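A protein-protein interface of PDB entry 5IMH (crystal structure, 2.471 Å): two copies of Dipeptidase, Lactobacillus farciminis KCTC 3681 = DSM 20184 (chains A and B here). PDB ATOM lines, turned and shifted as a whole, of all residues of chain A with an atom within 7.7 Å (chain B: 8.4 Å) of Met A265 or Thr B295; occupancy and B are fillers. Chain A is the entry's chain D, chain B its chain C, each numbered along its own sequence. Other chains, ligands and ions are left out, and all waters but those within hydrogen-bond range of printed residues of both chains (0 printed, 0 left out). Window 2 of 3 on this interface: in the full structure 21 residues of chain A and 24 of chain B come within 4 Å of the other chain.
Position printed for both chains: 307. Of the 8 pairs that touch across the chains among the printed residues, none has its exchanged pair printed and touching as well.
The side-chain hydroxyl of Thr A241 sits at hydrogen-bond distance from the side-chain amide oxygen of Asn B294, at 3.0 Å. O of Gly B303 lies close to O of Ser A306.
OG1 of Thr A241 sits at hydrogen-bond distance from O of Ile A238 (2.5 Å). O of Met A265 sits at hydrogen-bond distance from ND2 of Asn A245 (2.9 Å). N of Met A265 sits at hydrogen-bond distance from OD1 of Asp A263 (2.9 Å).
Ile A238 touches Glu B293 (CD1 to O, 3.4 Å). Asn B294 touches Ile A238 (OD1 to CG2, 3.5 Å). SD of Met A265 touches CB of Asn B294, 3.6 Å away. CE of Met A265 touches CG2 of Thr B295, at 3.7 Å. O of Ser B302 touches O of Ser A306 (3.997 Å). Leu A310 touches Ser B302.
Of the 13 printed residues of chain B, 5 touch a printed residue of chain A. Printed residues of chain B that touch a printed residue of chain A: Glu B293, Asn B294, Thr B295, Ser B302 and Gly B303. Hydrophobic or aromatic side chains of chain A within 4 Å of the printed part of chain B: Ile A238, Met A265 and Leu A310. Among the printed residues, 8 pairs touch across the chains. Among the printed residues, no Asp or Glu carboxylate lies within 4 Å of a Lys or Arg side-chain nitrogen of the other chain.
Printed residues of chain B within 4 Å of Ile A238: Glu B293 (3.4 Å) and Asn B294 (3.5 Å). Of the printed residues of chain B, Thr A241 touches Asn B294 (3.0 Å). No residue of chain B comes within 4 Å of Pro A264. Of chain B, only Asn B294 and Thr B295 come within 4 Å of Met A265. Printed residues of chain B within 4 Å of Ser A306: Ser B302 and Gly B303. Printed residues of chain A within 4 Å of Glu B293: Ile A238. Of chain A, only Met A265 (3.7 Å) comes within 4 Å of Thr B295. Of the printed residues of chain A, Gly B303 touches Ser A306 (2.8 Å). The nearest residue of chain B that does not touch Met A265 is Lys B296 (6.3 Å). The nearest printed residue of chain A that does not touch Thr B295 is Asp A307 (6.1 Å). The nearest printed residue of chain B that does not touch Ser A306 is Ser B304 (4.7 Å).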
ATOM      1  N   ARG A 192      12.275  -0.845  32.124  1.00  0.00           N
ATOM      2  CA  ARG A 192      13.639  -1.115  32.523  1.00  0.00           C
ATOM      3  C   ARG A 192      13.882  -0.290  33.764  1.00  0.00           C
ATOM      4  O   ARG A 192      13.457   0.868  33.817  1.00  0.00           O
ATOM      5  CB  ARG A 192      14.614  -0.748  31.401  1.00  0.00           C
ATOM      6  CG  ARG A 192      16.062  -1.012  31.703  1.00  0.00           C
ATOM      7  CD  ARG A 192      16.942  -0.580  30.533  1.00  0.00           C
ATOM      8  NE  ARG A 192      18.361  -0.638  30.879  1.00  0.00           N
ATOM      9  CZ  ARG A 192      19.233   0.325  30.606  1.00  0.00           C
ATOM     10  NH1 ARG A 192      18.836   1.400  29.944  1.00  0.00           N
ATOM     11  NH2 ARG A 192      20.511   0.204  30.963  1.00  0.00           N
ATOM     12  N   SER A 237      20.757  -5.017  29.260  1.00  0.00           N
ATOM     13  CA  SER A 237      20.743  -6.224  28.422  1.00  0.00           C
ATOM     14  C   SER A 237      20.567  -5.945  26.921  1.00  0.00           C
ATOM     15  O   SER A 237      20.262  -4.816  26.510  1.00  0.00           O
ATOM     16  CB  SER A 237      19.619  -7.160  28.864  1.00  0.00           C
ATOM     17  OG  SER A 237      18.378  -6.662  28.395  1.00  0.00           O
ATOM     18  N   ILE A 238      20.706  -7.005  26.123  1.00  0.00           N
ATOM     19  CA  ILE A 238      20.431  -6.957  24.695  1.00  0.00           C
ATOM     20  C   ILE A 238      18.954  -6.568  24.440  1.00  0.00           C
ATOM     21  O   ILE A 238      18.661  -5.746  23.564  1.00  0.00           O
ATOM     22  CB  ILE A 238      20.742  -8.320  24.027  1.00  0.00           C
ATOM     23  CG1 ILE A 238      22.213  -8.693  24.212  1.00  0.00           C
ATOM     24  CG2 ILE A 238      20.410  -8.285  22.547  1.00  0.00           C
ATOM     25  CD1 ILE A 238      23.163  -7.679  23.612  1.00  0.00           C
ATOM     26  N   ASP A 240      17.047  -4.738  26.374  1.00  0.00           N
ATOM     27  CA  ASP A 240      16.907  -3.317  26.724  1.00  0.00           C
ATOM     28  C   ASP A 240      17.173  -2.417  25.526  1.00  0.00           C
ATOM     29  O   ASP A 240      16.488  -1.404  25.338  1.00  0.00           O
ATOM     30  CB  ASP A 240      17.859  -2.928  27.879  1.00  0.00           C
ATOM     31  CG  ASP A 240      17.420  -3.487  29.227  1.00  0.00           C
ATOM     32  OD1 ASP A 240      16.193  -3.679  29.436  1.00  0.00           O
ATOM     33  OD2 ASP A 240      18.304  -3.705  30.089  1.00  0.00           O
ATOM     34  N   THR A 241      18.175  -2.791  24.728  1.00  0.00           N
ATOM     35  CA  THR A 241      18.625  -1.972  23.607  1.00  0.00           C
ATOM     36  C   THR A 241      17.546  -1.828  22.545  1.00  0.00           C
ATOM     37  O   THR A 241      17.558  -0.874  21.771  1.00  0.00           O
ATOM     38  CB  THR A 241      19.878  -2.562  22.915  1.00  0.00           C
ATOM     39  OG1 THR A 241      19.517  -3.773  22.238  1.00  0.00           O
ATOM     40  CG2 THR A 241      21.009  -2.826  23.917  1.00  0.00           C
ATOM     41  N   VAL A 242      16.633  -2.788  22.475  1.00  0.00           N
ATOM     42  CA  VAL A 242      15.600  -2.725  21.441  1.00  0.00           C
ATOM     43  C   VAL A 242      14.183  -2.525  21.984  1.00  0.00           C
ATOM     44  O   VAL A 242      13.313  -1.968  21.318  1.00  0.00           O
ATOM     45  CB  VAL A 242      15.638  -4.000  20.545  1.00  0.00           C
ATOM     46  CG1 VAL A 242      17.026  -4.192  19.945  1.00  0.00           C
ATOM     47  CG2 VAL A 242      15.205  -5.245  21.289  1.00  0.00           C
ATOM     48  N   ASN A 244      13.425  -1.241  25.245  1.00  0.00           N
ATOM     49  CA  ASN A 244      13.268  -0.182  26.254  1.00  0.00           C
ATOM     50  C   ASN A 244      13.903   1.155  25.866  1.00  0.00           C
ATOM     51  O   ASN A 244      13.206   2.170  25.737  1.00  0.00           O
ATOM     52  CB  ASN A 244      13.854  -0.651  27.595  1.00  0.00           C
ATOM     53  CG  ASN A 244      13.030  -1.745  28.239  1.00  0.00           C
ATOM     54  OD1 ASN A 244      11.803  -1.695  28.236  1.00  0.00           O
ATOM     55  ND2 ASN A 244      13.701  -2.749  28.784  1.00  0.00           N
ATOM     56  N   ASN A 245      15.226   1.144  25.678  1.00  0.00           N
ATOM     57  CA  ASN A 245      15.994   2.348  25.369  1.00  0.00           C
ATOM     58  C   ASN A 245      15.469   3.218  24.217  1.00  0.00           C
ATOM     59  O   ASN A 245      15.465   4.442  24.348  1.00  0.00           O
ATOM     60  CB  ASN A 245      17.457   1.959  25.089  1.00  0.00           C
ATOM     61  CG  ASN A 245      18.101   1.223  26.262  1.00  0.00           C
ATOM     62  OD1 ASN A 245      17.605   1.283  27.386  1.00  0.00           O
ATOM     63  ND2 ASN A 245      19.186   0.502  25.995  1.00  0.00           N
ATOM     64  N   PRO A 246      15.007   2.613  23.093  1.00  0.00           N
ATOM     65  CA  PRO A 246      14.470   3.475  22.024  1.00  0.00           C
ATOM     66  C   PRO A 246      13.219   4.278  22.446  1.00  0.00           C
ATOM     67  O   PRO A 246      12.961   5.363  21.913  1.00  0.00           O
ATOM     68  CB  PRO A 246      14.141   2.481  20.904  1.00  0.00           C
ATOM     69  CG  PRO A 246      15.018   1.312  21.155  1.00  0.00           C
ATOM     70  CD  PRO A 246      15.093   1.204  22.650  1.00  0.00           C
ATOM     71  N   TRP A 249      14.736   7.101  24.456  1.00  0.00           N
ATOM     72  CA  TRP A 249      15.406   7.971  23.502  1.00  0.00           C
ATOM     73  C   TRP A 249      14.427   8.837  22.719  1.00  0.00           C
ATOM     74  O   TRP A 249      14.573  10.057  22.637  1.00  0.00           O
ATOM     75  CB  TRP A 249      16.245   7.132  22.541  1.00  0.00           C
ATOM     76  CG  TRP A 249      16.856   7.938  21.471  1.00  0.00           C
ATOM     77  CD1 TRP A 249      18.032   8.650  21.544  1.00  0.00           C
ATOM     78  CD2 TRP A 249      16.352   8.126  20.149  1.00  0.00           C
ATOM     79  NE1 TRP A 249      18.280   9.275  20.340  1.00  0.00           N
ATOM     80  CE2 TRP A 249      17.269   8.961  19.467  1.00  0.00           C
ATOM     81  CE3 TRP A 249      15.228   7.658  19.467  1.00  0.00           C
ATOM     82  CZ2 TRP A 249      17.075   9.350  18.140  1.00  0.00           C
ATOM     83  CZ3 TRP A 249      15.039   8.046  18.149  1.00  0.00           C
ATOM     84  CH2 TRP A 249      15.958   8.878  17.499  1.00  0.00           C
ATOM     85  N   ASP A 262      22.227  10.404  18.993  1.00  0.00           N
ATOM     86  CA  ASP A 262      21.488   9.769  17.926  1.00  0.00           C
ATOM     87  C   ASP A 262      21.540   8.246  17.966  1.00  0.00           C
ATOM     88  O   ASP A 262      21.289   7.588  16.969  1.00  0.00           O
ATOM     89  CB  ASP A 262      21.996  10.323  16.602  1.00  0.00           C
ATOM     90  CG  ASP A 262      21.782  11.829  16.501  1.00  0.00           C
ATOM     91  OD1 ASP A 262      20.642  12.288  16.746  1.00  0.00           O
ATOM     92  OD2 ASP A 262      22.741  12.561  16.204  1.00  0.00           O
ATOM     93  N   ASP A 263      21.841   7.699  19.136  1.00  0.00           N
ATOM     94  CA  ASP A 263      21.845   6.260  19.345  1.00  0.00           C
ATOM     95  C   ASP A 263      20.661   5.870  20.245  1.00  0.00           C
ATOM     96  O   ASP A 263      20.728   6.059  21.459  1.00  0.00           O
ATOM     97  CB  ASP A 263      23.188   5.819  19.954  1.00  0.00           C
ATOM     98  CG  ASP A 263      23.257   4.310  20.225  1.00  0.00           C
ATOM     99  OD1 ASP A 263      22.359   3.574  19.771  1.00  0.00           O
ATOM    100  OD2 ASP A 263      24.226   3.852  20.884  1.00  0.00           O
ATOM    101  N   PRO A 264      19.569   5.335  19.644  1.00  0.00           N
ATOM    102  CA  PRO A 264      18.388   4.875  20.401  1.00  0.00           C
ATOM    103  C   PRO A 264      18.682   3.645  21.268  1.00  0.00           C
ATOM    104  O   PRO A 264      17.860   3.256  22.099  1.00  0.00           O
ATOM    105  CB  PRO A 264      17.363   4.518  19.305  1.00  0.00           C
ATOM    106  CG  PRO A 264      17.865   5.171  18.058  1.00  0.00           C
ATOM    107  CD  PRO A 264      19.375   5.172  18.190  1.00  0.00           C
ATOM    108  N   MET A 265      19.841   3.030  21.072  1.00  0.00           N
ATOM    109  CA  MET A 265      20.169   1.821  21.818  1.00  0.00           C
ATOM    110  C   MET A 265      20.915   2.123  23.115  1.00  0.00           C
ATOM    111  O   MET A 265      21.042   1.253  23.965  1.00  0.00           O
ATOM    112  CB  MET A 265      21.005   0.869  20.979  1.00  0.00           C
ATOM    113  CG  MET A 265      20.287   0.273  19.800  1.00  0.00           C
ATOM    114  SD  MET A 265      21.143  -1.175  19.128  1.00  0.00           S
ATOM    115  CE  MET A 265      22.771  -0.489  18.792  1.00  0.00           C
ATOM    116  N   GLU A 266      21.398   3.356  23.241  1.00  0.00           N
ATOM    117  CA  GLU A 266      22.182   3.822  24.390  1.00  0.00           C
ATOM    118  C   GLU A 266      21.693   3.312  25.758  1.00  0.00           C
ATOM    119  O   GLU A 266      20.545   3.500  26.107  1.00  0.00           O
ATOM    120  CB  GLU A 266      22.201   5.356  24.380  1.00  0.00           C
ATOM    121  CG  GLU A 266      22.868   5.960  25.577  1.00  0.00           C
ATOM    122  CD  GLU A 266      24.253   5.424  25.740  1.00  0.00           C
ATOM    123  OE1 GLU A 266      25.034   5.518  24.768  1.00  0.00           O
ATOM    124  OE2 GLU A 266      24.542   4.876  26.825  1.00  0.00           O
ATOM    125  N   GLN A 267      22.568   2.643  26.509  1.00  0.00           N
ATOM    126  CA  GLN A 267      22.197   2.063  27.800  1.00  0.00           C
ATOM    127  C   GLN A 267      22.209   3.072  28.977  1.00  0.00           C
ATOM    128  O   GLN A 267      21.634   2.807  30.057  1.00  0.00           O
ATOM    129  CB  GLN A 267      23.116   0.885  28.144  1.00  0.00           C
ATOM    130  CG  GLN A 267      23.049  -0.278  27.182  1.00  0.00           C
ATOM    131  CD  GLN A 267      21.892  -1.233  27.474  1.00  0.00           C
ATOM    132  OE1 GLN A 267      20.864  -0.838  28.034  1.00  0.00           O
ATOM    133  NE2 GLN A 267      22.047  -2.488  27.070  1.00  0.00           N
ATOM    134  N   ASP A 268      22.875   4.210  28.780  1.00  0.00           N
ATOM    135  CA  ASP A 268      22.998   5.204  29.849  1.00  0.00           C
ATOM    136  C   ASP A 268      22.350   6.524  29.506  1.00  0.00           C
ATOM    137  O   ASP A 268      22.889   7.568  29.833  1.00  0.00           O
ATOM    138  CB  ASP A 268      24.471   5.441  30.208  1.00  0.00           C
ATOM    139  CG  ASP A 268      25.120   4.215  30.834  1.00  0.00           C
ATOM    140  OD1 ASP A 268      24.615   3.726  31.873  1.00  0.00           O
ATOM    141  OD2 ASP A 268      26.124   3.716  30.276  1.00  0.00           O
ATOM    142  N   LEU A 269      21.208   6.489  28.840  1.00  0.00           N
ATOM    143  CA  LEU A 269      20.411   7.705  28.735  1.00  0.00           C
ATOM    144  C   LEU A 269      20.083   8.166  30.147  1.00  0.00           C
ATOM    145  O   LEU A 269      19.839   7.341  31.024  1.00  0.00           O
ATOM    146  CB  LEU A 269      19.130   7.494  27.915  1.00  0.00           C
ATOM    147  CG  LEU A 269      19.403   7.232  26.426  1.00  0.00           C
ATOM    148  CD1 LEU A 269      18.141   6.825  25.721  1.00  0.00           C
ATOM    149  CD2 LEU A 269      19.989   8.480  25.772  1.00  0.00           C
ATOM    150  N   SER A 306      15.551  -0.879   5.350  1.00  0.00           N
ATOM    151  CA  SER A 306      16.788  -1.534   5.752  1.00  0.00           C
ATOM    152  C   SER A 306      16.956  -1.418   7.270  1.00  0.00           C
ATOM    153  O   SER A 306      17.693  -2.189   7.876  1.00  0.00           O
ATOM    154  CB  SER A 306      17.978  -0.905   5.018  1.00  0.00           C
ATOM    155  OG  SER A 306      17.819   0.492   4.902  1.00  0.00           O
ATOM    156  N   ASP A 307      16.268  -0.439   7.860  1.00  0.00           N
ATOM    157  CA  ASP A 307      16.132  -0.294   9.314  1.00  0.00           C
ATOM    158  C   ASP A 307      14.701  -0.645   9.761  1.00  0.00           C
ATOM    159  O   ASP A 307      13.856   0.244   9.909  1.00  0.00           O
ATOM    160  CB  ASP A 307      16.514   1.122   9.773  1.00  0.00           C
ATOM    161  CG  ASP A 307      18.022   1.301   9.918  1.00  0.00           C
ATOM    162  OD1 ASP A 307      18.782   0.602   9.208  1.00  0.00           O
ATOM    163  OD2 ASP A 307      18.452   2.153  10.723  1.00  0.00           O
ATOM    164  N   LEU A 310      13.270  -5.140  14.892  1.00  0.00           N
ATOM    165  CA  LEU A 310      13.211  -5.097  16.349  1.00  0.00           C
ATOM    166  C   LEU A 310      13.518  -3.828  17.168  1.00  0.00           C
ATOM    167  O   LEU A 310      14.239  -3.921  18.131  1.00  0.00           O
ATOM    168  CB  LEU A 310      14.111  -6.231  16.884  1.00  0.00           C
ATOM    169  CG  LEU A 310      15.547  -6.468  16.379  1.00  0.00           C
ATOM    170  CD1 LEU A 310      16.520  -5.298  16.568  1.00  0.00           C
ATOM    171  CD2 LEU A 310      16.123  -7.751  16.989  1.00  0.00           C
ATOM    172  N   PHE A 311      12.961  -2.662  16.849  1.00  0.00           N
ATOM    173  CA  PHE A 311      12.948  -1.575  17.856  1.00  0.00           C
ATOM    174  C   PHE A 311      11.477  -1.453  18.262  1.00  0.00           C
ATOM    175  O   PHE A 311      10.617  -1.983  17.599  1.00  0.00           O
ATOM    176  CB  PHE A 311      13.529  -0.241  17.386  1.00  0.00           C
ATOM    177  CG  PHE A 311      15.026  -0.158  17.485  1.00  0.00           C
ATOM    178  CD1 PHE A 311      15.744  -1.162  18.116  1.00  0.00           C
ATOM    179  CD2 PHE A 311      15.706   0.971  17.042  1.00  0.00           C
ATOM    180  CE1 PHE A 311      17.118  -1.081  18.239  1.00  0.00           C
ATOM    181  CE2 PHE A 311      17.077   1.057  17.167  1.00  0.00           C
ATOM    182  CZ  PHE A 311      17.778   0.031  17.761  1.00  0.00           C
ATOM    183  N   PHE B 292      28.095 -11.075  18.571  1.00  0.00           N
ATOM    184  CA  PHE B 292      28.157  -9.749  17.936  1.00  0.00           C
ATOM    185  C   PHE B 292      26.733  -9.204  17.756  1.00  0.00           C
ATOM    186  O   PHE B 292      26.370  -8.819  16.641  1.00  0.00           O
ATOM    187  CB  PHE B 292      28.831  -9.766  16.555  1.00  0.00           C
ATOM    188  CG  PHE B 292      30.225 -10.296  16.537  1.00  0.00           C
ATOM    189  CD1 PHE B 292      31.160  -9.889  17.462  1.00  0.00           C
ATOM    190  CD2 PHE B 292      30.604 -11.197  15.555  1.00  0.00           C
ATOM    191  CE1 PHE B 292      32.446 -10.375  17.416  1.00  0.00           C
ATOM    192  CE2 PHE B 292      31.889 -11.685  15.506  1.00  0.00           C
ATOM    193  CZ  PHE B 292      32.813 -11.279  16.443  1.00  0.00           C
ATOM    194  N   GLU B 293      25.913  -9.172  18.813  1.00  0.00           N
ATOM    195  CA  GLU B 293      24.500  -8.844  18.593  1.00  0.00           C
ATOM    196  C   GLU B 293      24.157  -7.476  19.142  1.00  0.00           C
ATOM    197  O   GLU B 293      24.087  -7.302  20.354  1.00  0.00           O
ATOM    198  CB  GLU B 293      23.528  -9.810  19.264  1.00  0.00           C
ATOM    199  CG  GLU B 293      23.330 -11.149  18.630  1.00  0.00           C
ATOM    200  CD  GLU B 293      24.162 -12.162  19.356  1.00  0.00           C
ATOM    201  OE1 GLU B 293      24.938 -11.717  20.235  1.00  0.00           O
ATOM    202  OE2 GLU B 293      24.008 -13.380  19.112  1.00  0.00           O
ATOM    203  N   ASN B 294      24.152  -6.492  18.253  1.00  0.00           N
ATOM    204  CA  ASN B 294      23.032  -5.581  17.948  1.00  0.00           C
ATOM    205  C   ASN B 294      23.389  -5.048  16.570  1.00  0.00           C
ATOM    206  O   ASN B 294      24.152  -5.689  15.843  1.00  0.00           O
ATOM    207  CB  ASN B 294      22.749  -4.447  18.964  1.00  0.00           C
ATOM    208  CG  ASN B 294      22.593  -4.932  20.407  1.00  0.00           C
ATOM    209  OD1 ASN B 294      21.521  -5.413  20.786  1.00  0.00           O
ATOM    210  ND2 ASN B 294      23.609  -4.716  21.232  1.00  0.00           N
ATOM    211  N   THR B 295      22.889  -3.863  16.234  1.00  0.00           N
ATOM    212  CA  THR B 295      22.870  -3.312  14.861  1.00  0.00           C
ATOM    213  C   THR B 295      23.986  -3.707  13.857  1.00  0.00           C
ATOM    214  O   THR B 295      23.817  -3.525  12.652  1.00  0.00           O
ATOM    215  CB  THR B 295      22.866  -1.759  14.920  1.00  0.00           C
ATOM    216  OG1 THR B 295      22.601  -1.226  13.618  1.00  0.00           O
ATOM    217  CG2 THR B 295      24.208  -1.231  15.415  1.00  0.00           C
ATOM    218  N   LYS B 296      25.130  -4.191  14.336  1.00  0.00           N
ATOM    219  CA  LYS B 296      26.290  -4.348  13.452  1.00  0.00           C
ATOM    220  C   LYS B 296      26.462  -5.651  12.591  1.00  0.00           C
ATOM    221  O   LYS B 296      26.216  -5.621  11.380  1.00  0.00           O
ATOM    222  CB  LYS B 296      27.530  -4.129  14.341  1.00  0.00           C
ATOM    223  CG  LYS B 296      27.595  -5.072  15.540  1.00  0.00           C
ATOM    224  CD  LYS B 296      28.638  -4.686  16.551  1.00  0.00           C
ATOM    225  CE  LYS B 296      28.731  -5.768  17.596  1.00  0.00           C
ATOM    226  NZ  LYS B 296      29.451  -6.888  16.908  1.00  0.00           N
ATOM    227  N   TYR B 297      26.897  -6.752  13.214  1.00  0.00           N
ATOM    228  CA  TYR B 297      27.287  -8.022  12.557  1.00  0.00           C
ATOM    229  C   TYR B 297      26.779  -9.273  13.324  1.00  0.00           C
ATOM    230  O   TYR B 297      27.497  -9.824  14.127  1.00  0.00           O
ATOM    231  CB  TYR B 297      28.823  -8.094  12.424  1.00  0.00           C
ATOM    232  CG  TYR B 297      29.426  -7.858  11.043  1.00  0.00           C
ATOM    233  CD1 TYR B 297      29.881  -8.924  10.261  1.00  0.00           C
ATOM    234  CD2 TYR B 297      29.555  -6.568  10.531  1.00  0.00           C
ATOM    235  CE1 TYR B 297      30.452  -8.704   9.005  1.00  0.00           C
ATOM    236  CE2 TYR B 297      30.115  -6.340   9.283  1.00  0.00           C
ATOM    237  CZ  TYR B 297      30.559  -7.410   8.522  1.00  0.00           C
ATOM    238  OH  TYR B 297      31.114  -7.184   7.280  1.00  0.00           O
ATOM    239  N   ASP B 298      25.583  -9.755  13.029  1.00  0.00           N
ATOM    240  CA  ASP B 298      24.951 -10.885  13.717  1.00  0.00           C
ATOM    241  C   ASP B 298      25.185 -12.134  12.844  1.00  0.00           C
ATOM    242  O   ASP B 298      26.018 -12.078  11.946  1.00  0.00           O
ATOM    243  CB  ASP B 298      23.457 -10.561  13.897  1.00  0.00           C
ATOM    244  CG  ASP B 298      22.661 -11.639  14.633  1.00  0.00           C
ATOM    245  OD1 ASP B 298      23.089 -12.811  14.692  1.00  0.00           O
ATOM    246  OD2 ASP B 298      21.544 -11.309  15.106  1.00  0.00           O
ATOM    247  N   GLY B 301      20.828 -11.509  11.413  1.00  0.00           N
ATOM    248  CA  GLY B 301      19.935 -10.581  12.110  1.00  0.00           C
ATOM    249  C   GLY B 301      18.945  -9.773  11.260  1.00  0.00           C
ATOM    250  O   GLY B 301      18.113 -10.348  10.541  1.00  0.00           O
ATOM    251  N   SER B 302      19.015  -8.438  11.346  1.00  0.00           N
ATOM    252  CA  SER B 302      17.949  -7.604  10.777  1.00  0.00           C
ATOM    253  C   SER B 302      18.310  -6.677   9.592  1.00  0.00           C
ATOM    254  O   SER B 302      17.421  -5.990   9.082  1.00  0.00           O
ATOM    255  CB  SER B 302      17.329  -6.739  11.891  1.00  0.00           C
ATOM    256  OG  SER B 302      17.182  -7.458  13.109  1.00  0.00           O
ATOM    257  N   GLY B 303      19.573  -6.616   9.157  1.00  0.00           N
ATOM    258  CA  GLY B 303      19.886  -5.879   7.931  1.00  0.00           C
ATOM    259  C   GLY B 303      20.600  -4.530   7.869  1.00  0.00           C
ATOM    260  O   GLY B 303      20.058  -3.574   8.436  1.00  0.00           O
ATOM    261  N   SER B 304      21.799  -4.397   7.271  1.00  0.00           N
ATOM    262  CA  SER B 304      22.721  -5.412   6.685  1.00  0.00           C
ATOM    263  C   SER B 304      22.337  -6.577   5.717  1.00  0.00           C
ATOM    264  O   SER B 304      21.258  -7.152   5.803  1.00  0.00           O
ATOM    265  CB  SER B 304      23.433  -6.069   7.884  1.00  0.00           C
ATOM    266  OG  SER B 304      24.479  -6.949   7.494  1.00  0.00           O
ATOM    267  N   ASP B 307      27.142  -7.059   5.237  1.00  0.00           N
ATOM    268  CA  ASP B 307      27.729  -7.161   6.570  1.00  0.00           C
ATOM    269  C   ASP B 307      27.489  -8.412   7.445  1.00  0.00           C
ATOM    270  O   ASP B 307      27.650  -8.257   8.639  1.00  0.00           O
ATOM    271  CB  ASP B 307      27.254  -5.949   7.415  1.00  0.00           C
ATOM    272  CG  ASP B 307      27.668  -4.584   6.825  1.00  0.00           C
ATOM    273  OD1 ASP B 307      28.879  -4.262   6.731  1.00  0.00           O
ATOM    274  OD2 ASP B 307      26.740  -3.829   6.452  1.00  0.00           O
ATOM    275  N   LYS B 308      27.093  -9.591   6.938  1.00  0.00           N
ATOM    276  CA  LYS B 308      27.383 -10.863   7.659  1.00  0.00           C
ATOM    277  C   LYS B 308      27.573 -11.981   6.654  1.00  0.00           C
ATOM    278  O   LYS B 308      26.751 -12.137   5.762  1.00  0.00           O
ATOM    279  CB  LYS B 308      26.313 -11.234   8.697  1.00  0.00           C
ATOM    280  CG  LYS B 308      25.902 -10.039   9.514  1.00  0.00           C
ATOM    281  CD  LYS B 308      24.578 -10.102  10.091  1.00  0.00           C
ATOM    282  CE  LYS B 308      24.116  -8.766  10.624  1.00  0.00           C
ATOM    283  NZ  LYS B 308      22.722  -8.882  11.027  1.00  0.00           N
